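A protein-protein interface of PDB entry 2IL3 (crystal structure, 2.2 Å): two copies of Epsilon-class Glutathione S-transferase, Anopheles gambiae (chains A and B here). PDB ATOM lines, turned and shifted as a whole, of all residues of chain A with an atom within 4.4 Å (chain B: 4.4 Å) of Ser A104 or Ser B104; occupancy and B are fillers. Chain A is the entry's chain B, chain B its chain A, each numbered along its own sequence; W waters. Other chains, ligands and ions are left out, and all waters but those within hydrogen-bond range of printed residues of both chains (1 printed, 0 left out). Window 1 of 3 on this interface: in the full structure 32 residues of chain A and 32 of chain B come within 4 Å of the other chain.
Ser A104 touches just these residues of chain B: His B101, Ser B104 and Gly B105. Printed residues of chain B within 4 Å of Ala A109: Gly B105 (3.95 Å) and Ala B109 (3.7 Å). Of the printed residues of chain A, His B69 touches His A101. Of the printed residues of chain A, Leu B100 touches His A101. Of chain A, only His A101, Ser A104 and Gly A105 come within 4 Å of Ser B104. The nearest printed residue of chain A that does not touch Leu B100 is Ser A104 (5.9 Å).
NE2 of His B101 lies within hydrogen-bond range of NE2 of His A101 (3.3 Å). A ring nitrogen (ND1) of His A101 lies within hydrogen-bond range of the side-chain hydroxyl (OG) of Ser B104 (2.5 Å). ND1 of His B101 lies within hydrogen-bond range of OG of Ser A104, 2.8 Å away.
Leu A100 touches His B101, and with the chains exchanged His A101 touches Leu B100. His B101 touches its own counterpart, His A101. His A101 touches Ser B104, and with the chains exchanged Ser A104 touches His B101. Gly A105 touches Ala B109, and with the chains exchanged Ala A109 touches Gly B105. Of the 13 pairs that touch across the chains among the printed residues, 13 have their exchanged pair printed and touching as well.
Hydrophobic or aromatic side chains of chain B that line the printed part of chain A: His B69, Leu B100, His B101 and Ala B109. Printed residues of chain A that touch a printed residue of chain B: His A69, Leu A100, His A101, Ser A104, Gly A105 and Ala A109. Hydrophobic or aromatic side chains of chain A within 4 Å of the printed part of chain B: His A69, Leu A100, His A101 and Ala A109. Among the printed residues, no Asp or Glu carboxylate lies within 4 Å of a Lys or Arg side-chain nitrogen of the other chain.
Water W1 bridges a ring nitrogen (NE2) of His A101 (2.9 Å) and a ring nitrogen (NE2) of His B101 (3.1 Å).
Among the printed residues, merely in contact across the chains: Gly A105 with Ser B104 (3.3 Å), Ser A104 with Gly B105 (3.3 Å), His A101 with Leu B100 (3.4 Å), His A101 with His B69 (3.4 Å), His A69 with His B101 (3.4 Å), Leu A100 with His B101 (3.7 Å), Ala A109 with Ala B109 (3.7 Å), Gly A105 with Ala B109 (3.8 Å), Ser A104 with Ser B104 (3.8 Å) and Ala A109 with Gly B105 (3.95 Å).
The side-chain hydroxyl (OG) of Ser B104 is in hydrogen-bond range of a ring nitrogen (NE2) of His B69, 3.0 Å away. O of Leu B100 is in hydrogen-bond range of OG of Ser B104, 3.2 Å away. The side-chain carboxylate of Glu B103 lies close to a ring nitrogen (NE2) of His B69, 3.4 Å away. The backbone carbonyl oxygen of Leu A100 sits at hydrogen-bond distance from the side-chain hydroxyl of Ser A104 (3.3 Å). NE2 of His A69 is in hydrogen-bond range of OE2 of Glu A103. The backbone carbonyl oxygen of Ser B104 lies within hydrogen-bond range of the backbone NH of Ala B109, 3.5 Å away.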
ATOM      1  N   HIS A  69     -21.325  -1.060 -31.128  1.00  0.00           N
ATOM      2  CA  HIS A  69     -22.305  -1.251 -29.998  1.00  0.00           C
ATOM      3  C   HIS A  69     -22.657   0.047 -29.304  1.00  0.00           C
ATOM      4  O   HIS A  69     -23.765   0.244 -28.907  1.00  0.00           O
ATOM      5  CB  HIS A  69     -21.914  -2.352 -28.987  1.00  0.00           C
ATOM      6  CG  HIS A  69     -21.407  -3.660 -29.600  1.00  0.00           C
ATOM      7  ND1 HIS A  69     -20.121  -3.814 -30.117  1.00  0.00           N
ATOM      8  CD2 HIS A  69     -21.958  -4.889 -29.629  1.00  0.00           C
ATOM      9  CE1 HIS A  69     -19.967  -5.059 -30.539  1.00  0.00           C
ATOM     10  NE2 HIS A  69     -21.070  -5.734 -30.248  1.00  0.00           N
ATOM     11  N   LEU A 100     -24.335  -8.120 -25.447  1.00  0.00           N
ATOM     12  CA  LEU A 100     -23.492  -7.199 -26.290  1.00  0.00           C
ATOM     13  C   LEU A 100     -21.960  -7.425 -26.048  1.00  0.00           C
ATOM     14  O   LEU A 100     -21.196  -7.508 -26.968  1.00  0.00           O
ATOM     15  CB  LEU A 100     -23.872  -5.733 -26.070  1.00  0.00           C
ATOM     16  CG  LEU A 100     -25.241  -5.113 -26.460  1.00  0.00           C
ATOM     17  CD1 LEU A 100     -25.346  -3.643 -25.838  1.00  0.00           C
ATOM     18  CD2 LEU A 100     -25.516  -5.133 -28.150  1.00  0.00           C
ATOM     19  N   HIS A 101     -21.521  -7.418 -24.805  1.00  0.00           N
ATOM     20  CA  HIS A 101     -20.195  -7.750 -24.485  1.00  0.00           C
ATOM     21  C   HIS A 101     -19.659  -9.204 -24.823  1.00  0.00           C
ATOM     22  O   HIS A 101     -18.515  -9.311 -25.270  1.00  0.00           O
ATOM     23  CB  HIS A 101     -19.947  -7.298 -23.067  1.00  0.00           C
ATOM     24  CG  HIS A 101     -19.766  -5.811 -22.943  1.00  0.00           C
ATOM     25  ND1 HIS A 101     -18.604  -5.173 -23.388  1.00  0.00           N
ATOM     26  CD2 HIS A 101     -20.639  -4.829 -22.561  1.00  0.00           C
ATOM     27  CE1 HIS A 101     -18.719  -3.879 -23.126  1.00  0.00           C
ATOM     28  NE2 HIS A 101     -19.945  -3.645 -22.672  1.00  0.00           N
ATOM     29  N   PHE A 102     -20.525 -10.246 -24.709  1.00  0.00           N
ATOM     30  CA  PHE A 102     -20.351 -11.615 -25.226  1.00  0.00           C
ATOM     31  C   PHE A 102     -20.152 -11.418 -26.707  1.00  0.00           C
ATOM     32  O   PHE A 102     -19.265 -12.023 -27.385  1.00  0.00           O
ATOM     33  CB  PHE A 102     -21.598 -12.542 -24.877  1.00  0.00           C
ATOM     34  CG  PHE A 102     -21.678 -13.835 -25.703  1.00  0.00           C
ATOM     35  CD1 PHE A 102     -20.713 -14.866 -25.533  1.00  0.00           C
ATOM     36  CD2 PHE A 102     -22.712 -14.014 -26.672  1.00  0.00           C
ATOM     37  CE1 PHE A 102     -20.743 -16.057 -26.291  1.00  0.00           C
ATOM     38  CE2 PHE A 102     -22.789 -15.213 -27.439  1.00  0.00           C
ATOM     39  CZ  PHE A 102     -21.783 -16.241 -27.259  1.00  0.00           C
ATOM     40  N   GLU A 103     -20.878 -10.449 -27.231  1.00  0.00           N
ATOM     41  CA  GLU A 103     -20.777 -10.305 -28.680  1.00  0.00           C
ATOM     42  C   GLU A 103     -19.476  -9.750 -29.150  1.00  0.00           C
ATOM     43  O   GLU A 103     -18.850 -10.287 -30.129  1.00  0.00           O
ATOM     44  CB  GLU A 103     -21.992  -9.632 -29.311  1.00  0.00           C
ATOM     45  CG  GLU A 103     -22.140  -9.982 -30.738  1.00  0.00           C
ATOM     46  CD  GLU A 103     -21.157  -9.338 -31.710  1.00  0.00           C
ATOM     47  OE1 GLU A 103     -20.959  -9.911 -32.805  1.00  0.00           O
ATOM     48  OE2 GLU A 103     -20.638  -8.237 -31.457  1.00  0.00           O
ATOM     49  N   SER A 104     -18.993  -8.683 -28.529  1.00  0.00           N
ATOM     50  CA  SER A 104     -17.675  -8.202 -29.006  1.00  0.00           C
ATOM     51  C   SER A 104     -16.535  -9.093 -28.541  1.00  0.00           C
ATOM     52  O   SER A 104     -15.587  -9.279 -29.276  1.00  0.00           O
ATOM     53  CB  SER A 104     -17.399  -6.766 -28.621  1.00  0.00           C
ATOM     54  OG  SER A 104     -18.177  -6.395 -27.542  1.00  0.00           O
ATOM     55  N   GLY A 105     -16.621  -9.617 -27.292  1.00  0.00           N
ATOM     56  CA  GLY A 105     -15.491 -10.314 -26.673  1.00  0.00           C
ATOM     57  C   GLY A 105     -15.288 -11.733 -27.163  1.00  0.00           C
ATOM     58  O   GLY A 105     -14.159 -12.282 -27.059  1.00  0.00           O
ATOM     59  N   VAL A 106     -16.346 -12.303 -27.756  1.00  0.00           N
ATOM     60  CA  VAL A 106     -16.393 -13.759 -28.168  1.00  0.00           C
ATOM     61  C   VAL A 106     -16.730 -13.979 -29.622  1.00  0.00           C
ATOM     62  O   VAL A 106     -15.905 -14.434 -30.395  1.00  0.00           O
ATOM     63  CB  VAL A 106     -17.321 -14.626 -27.223  1.00  0.00           C
ATOM     64  CG1 VAL A 106     -17.340 -16.086 -27.682  1.00  0.00           C
ATOM     65  CG2 VAL A 106     -16.830 -14.505 -25.761  1.00  0.00           C
ATOM     66  N   PHE A 108     -17.574 -11.770 -32.219  1.00  0.00           N
ATOM     67  CA  PHE A 108     -16.899 -10.995 -33.223  1.00  0.00           C
ATOM     68  C   PHE A 108     -15.396 -11.237 -33.285  1.00  0.00           C
ATOM     69  O   PHE A 108     -14.802 -11.351 -34.389  1.00  0.00           O
ATOM     70  CB  PHE A 108     -17.189  -9.529 -33.061  1.00  0.00           C
ATOM     71  CG  PHE A 108     -16.570  -8.710 -34.142  1.00  0.00           C
ATOM     72  CD1 PHE A 108     -15.521  -7.898 -33.883  1.00  0.00           C
ATOM     73  CD2 PHE A 108     -17.027  -8.800 -35.450  1.00  0.00           C
ATOM     74  CE1 PHE A 108     -14.954  -7.102 -34.906  1.00  0.00           C
ATOM     75  CE2 PHE A 108     -16.414  -8.047 -36.463  1.00  0.00           C
ATOM     76  CZ  PHE A 108     -15.365  -7.192 -36.164  1.00  0.00           C
ATOM     77  N   ALA A 109     -14.802 -11.271 -32.097  1.00  0.00           N
ATOM     78  CA  ALA A 109     -13.351 -11.367 -31.893  1.00  0.00           C
ATOM     79  C   ALA A 109     -12.776 -12.626 -32.565  1.00  0.00           C
ATOM     80  O   ALA A 109     -11.732 -12.572 -33.154  1.00  0.00           O
ATOM     81  CB  ALA A 109     -13.059 -11.371 -30.460  1.00  0.00           C
ATOM     82  N   HIS B  69     -18.828  -6.102 -17.665  1.00  0.00           N
ATOM     83  CA  HIS B  69     -19.042  -4.704 -18.103  1.00  0.00           C
ATOM     84  C   HIS B  69     -20.459  -4.354 -17.746  1.00  0.00           C
ATOM     85  O   HIS B  69     -20.717  -3.235 -17.294  1.00  0.00           O
ATOM     86  CB  HIS B  69     -18.773  -4.505 -19.591  1.00  0.00           C
ATOM     87  CG  HIS B  69     -17.418  -4.940 -19.993  1.00  0.00           C
ATOM     88  ND1 HIS B  69     -16.354  -4.071 -20.049  1.00  0.00           N
ATOM     89  CD2 HIS B  69     -16.925  -6.156 -20.302  1.00  0.00           C
ATOM     90  CE1 HIS B  69     -15.260  -4.724 -20.393  1.00  0.00           C
ATOM     91  NE2 HIS B  69     -15.577  -5.995 -20.550  1.00  0.00           N
ATOM     92  N   LEU B 100     -15.555   0.564 -23.570  1.00  0.00           N
ATOM     93  CA  LEU B 100     -15.899  -0.707 -22.905  1.00  0.00           C
ATOM     94  C   LEU B 100     -15.922  -1.852 -23.877  1.00  0.00           C
ATOM     95  O   LEU B 100     -15.516  -2.953 -23.517  1.00  0.00           O
ATOM     96  CB  LEU B 100     -17.194  -0.678 -22.143  1.00  0.00           C
ATOM     97  CG  LEU B 100     -17.154   0.111 -20.848  1.00  0.00           C
ATOM     98  CD1 LEU B 100     -18.634   0.447 -20.576  1.00  0.00           C
ATOM     99  CD2 LEU B 100     -16.413  -0.633 -19.672  1.00  0.00           C
ATOM    100  N   HIS B 101     -16.345  -1.579 -25.103  1.00  0.00           N
ATOM    101  CA  HIS B 101     -16.394  -2.555 -26.107  1.00  0.00           C
ATOM    102  C   HIS B 101     -15.138  -2.797 -26.832  1.00  0.00           C
ATOM    103  O   HIS B 101     -14.954  -3.871 -27.394  1.00  0.00           O
ATOM    104  CB  HIS B 101     -17.507  -2.249 -27.082  1.00  0.00           C
ATOM    105  CG  HIS B 101     -18.847  -2.651 -26.574  1.00  0.00           C
ATOM    106  ND1 HIS B 101     -19.250  -3.969 -26.553  1.00  0.00           N
ATOM    107  CD2 HIS B 101     -19.848  -1.926 -26.016  1.00  0.00           C
ATOM    108  CE1 HIS B 101     -20.479  -4.031 -26.069  1.00  0.00           C
ATOM    109  NE2 HIS B 101     -20.870  -2.804 -25.752  1.00  0.00           N
ATOM    110  N   PHE B 102     -14.283  -1.776 -26.847  1.00  0.00           N
ATOM    111  CA  PHE B 102     -12.900  -1.844 -27.292  1.00  0.00           C
ATOM    112  C   PHE B 102     -12.115  -2.770 -26.330  1.00  0.00           C
ATOM    113  O   PHE B 102     -11.476  -3.775 -26.738  1.00  0.00           O
ATOM    114  CB  PHE B 102     -12.308  -0.401 -27.366  1.00  0.00           C
ATOM    115  CG  PHE B 102     -10.799  -0.415 -27.474  1.00  0.00           C
ATOM    116  CD1 PHE B 102     -10.180  -0.847 -28.666  1.00  0.00           C
ATOM    117  CD2 PHE B 102      -9.996  -0.155 -26.342  1.00  0.00           C
ATOM    118  CE1 PHE B 102      -8.733  -0.952 -28.722  1.00  0.00           C
ATOM    119  CE2 PHE B 102      -8.604  -0.242 -26.401  1.00  0.00           C
ATOM    120  CZ  PHE B 102      -7.964  -0.645 -27.634  1.00  0.00           C
ATOM    121  N   GLU B 103     -12.181  -2.493 -25.040  1.00  0.00           N
ATOM    122  CA  GLU B 103     -11.717  -3.442 -24.071  1.00  0.00           C
ATOM    123  C   GLU B 103     -12.266  -4.877 -24.248  1.00  0.00           C
ATOM    124  O   GLU B 103     -11.448  -5.800 -24.303  1.00  0.00           O
ATOM    125  CB  GLU B 103     -12.052  -3.013 -22.662  1.00  0.00           C
ATOM    126  CG  GLU B 103     -10.954  -3.580 -21.669  1.00  0.00           C
ATOM    127  CD  GLU B 103     -11.165  -5.034 -21.140  1.00  0.00           C
ATOM    128  OE1 GLU B 103     -12.252  -5.556 -21.176  1.00  0.00           O
ATOM    129  OE2 GLU B 103     -10.226  -5.640 -20.571  1.00  0.00           O
ATOM    130  N   SER B 104     -13.587  -5.116 -24.319  1.00  0.00           N
ATOM    131  CA  SER B 104     -14.096  -6.494 -24.554  1.00  0.00           C
ATOM    132  C   SER B 104     -13.549  -7.143 -25.847  1.00  0.00           C
ATOM    133  O   SER B 104     -13.101  -8.269 -25.848  1.00  0.00           O
ATOM    134  CB  SER B 104     -15.609  -6.500 -24.683  1.00  0.00           C
ATOM    135  OG  SER B 104     -16.287  -6.060 -23.498  1.00  0.00           O
ATOM    136  N   GLY B 105     -13.579  -6.388 -26.949  1.00  0.00           N
ATOM    137  CA  GLY B 105     -13.442  -6.929 -28.248  1.00  0.00           C
ATOM    138  C   GLY B 105     -12.040  -6.936 -28.732  1.00  0.00           C
ATOM    139  O   GLY B 105     -11.693  -7.762 -29.604  1.00  0.00           O
ATOM    140  N   VAL B 106     -11.220  -6.034 -28.181  1.00  0.00           N
ATOM    141  CA  VAL B 106      -9.821  -5.986 -28.602  1.00  0.00           C
ATOM    142  C   VAL B 106      -8.829  -6.401 -27.556  1.00  0.00           C
ATOM    143  O   VAL B 106      -8.150  -7.341 -27.756  1.00  0.00           O
ATOM    144  CB  VAL B 106      -9.395  -4.584 -29.114  1.00  0.00           C
ATOM    145  CG1 VAL B 106      -7.978  -4.636 -29.660  1.00  0.00           C
ATOM    146  CG2 VAL B 106     -10.351  -4.227 -30.188  1.00  0.00           C
ATOM    147  N   PHE B 108      -9.072  -7.518 -24.245  1.00  0.00           N
ATOM    148  CA  PHE B 108      -9.260  -8.755 -23.447  1.00  0.00           C
ATOM    149  C   PHE B 108      -9.362  -9.952 -24.345  1.00  0.00           C
ATOM    150  O   PHE B 108      -8.866 -11.012 -24.010  1.00  0.00           O
ATOM    151  CB  PHE B 108     -10.449  -8.637 -22.494  1.00  0.00           C
ATOM    152  CG  PHE B 108     -10.990  -9.958 -21.946  1.00  0.00           C
ATOM    153  CD1 PHE B 108     -11.980 -10.677 -22.658  1.00  0.00           C
ATOM    154  CD2 PHE B 108     -10.557 -10.420 -20.687  1.00  0.00           C
ATOM    155  CE1 PHE B 108     -12.527 -11.881 -22.108  1.00  0.00           C
ATOM    156  CE2 PHE B 108     -11.028 -11.625 -20.145  1.00  0.00           C
ATOM    157  CZ  PHE B 108     -12.043 -12.356 -20.837  1.00  0.00           C
ATOM    158  N   ALA B 109      -9.992  -9.786 -25.490  1.00  0.00           N
ATOM    159  CA  ALA B 109     -10.111 -10.860 -26.438  1.00  0.00           C
ATOM    160  C   ALA B 109      -8.732 -11.340 -26.926  1.00  0.00           C
ATOM    161  O   ALA B 109      -8.506 -12.564 -27.034  1.00  0.00           O
ATOM    162  CB  ALA B 109     -10.937 -10.415 -27.608  1.00  0.00           C
HETATM  163  O   HOH W   1     -21.285  -1.144 -23.209  1.00  0.00           O
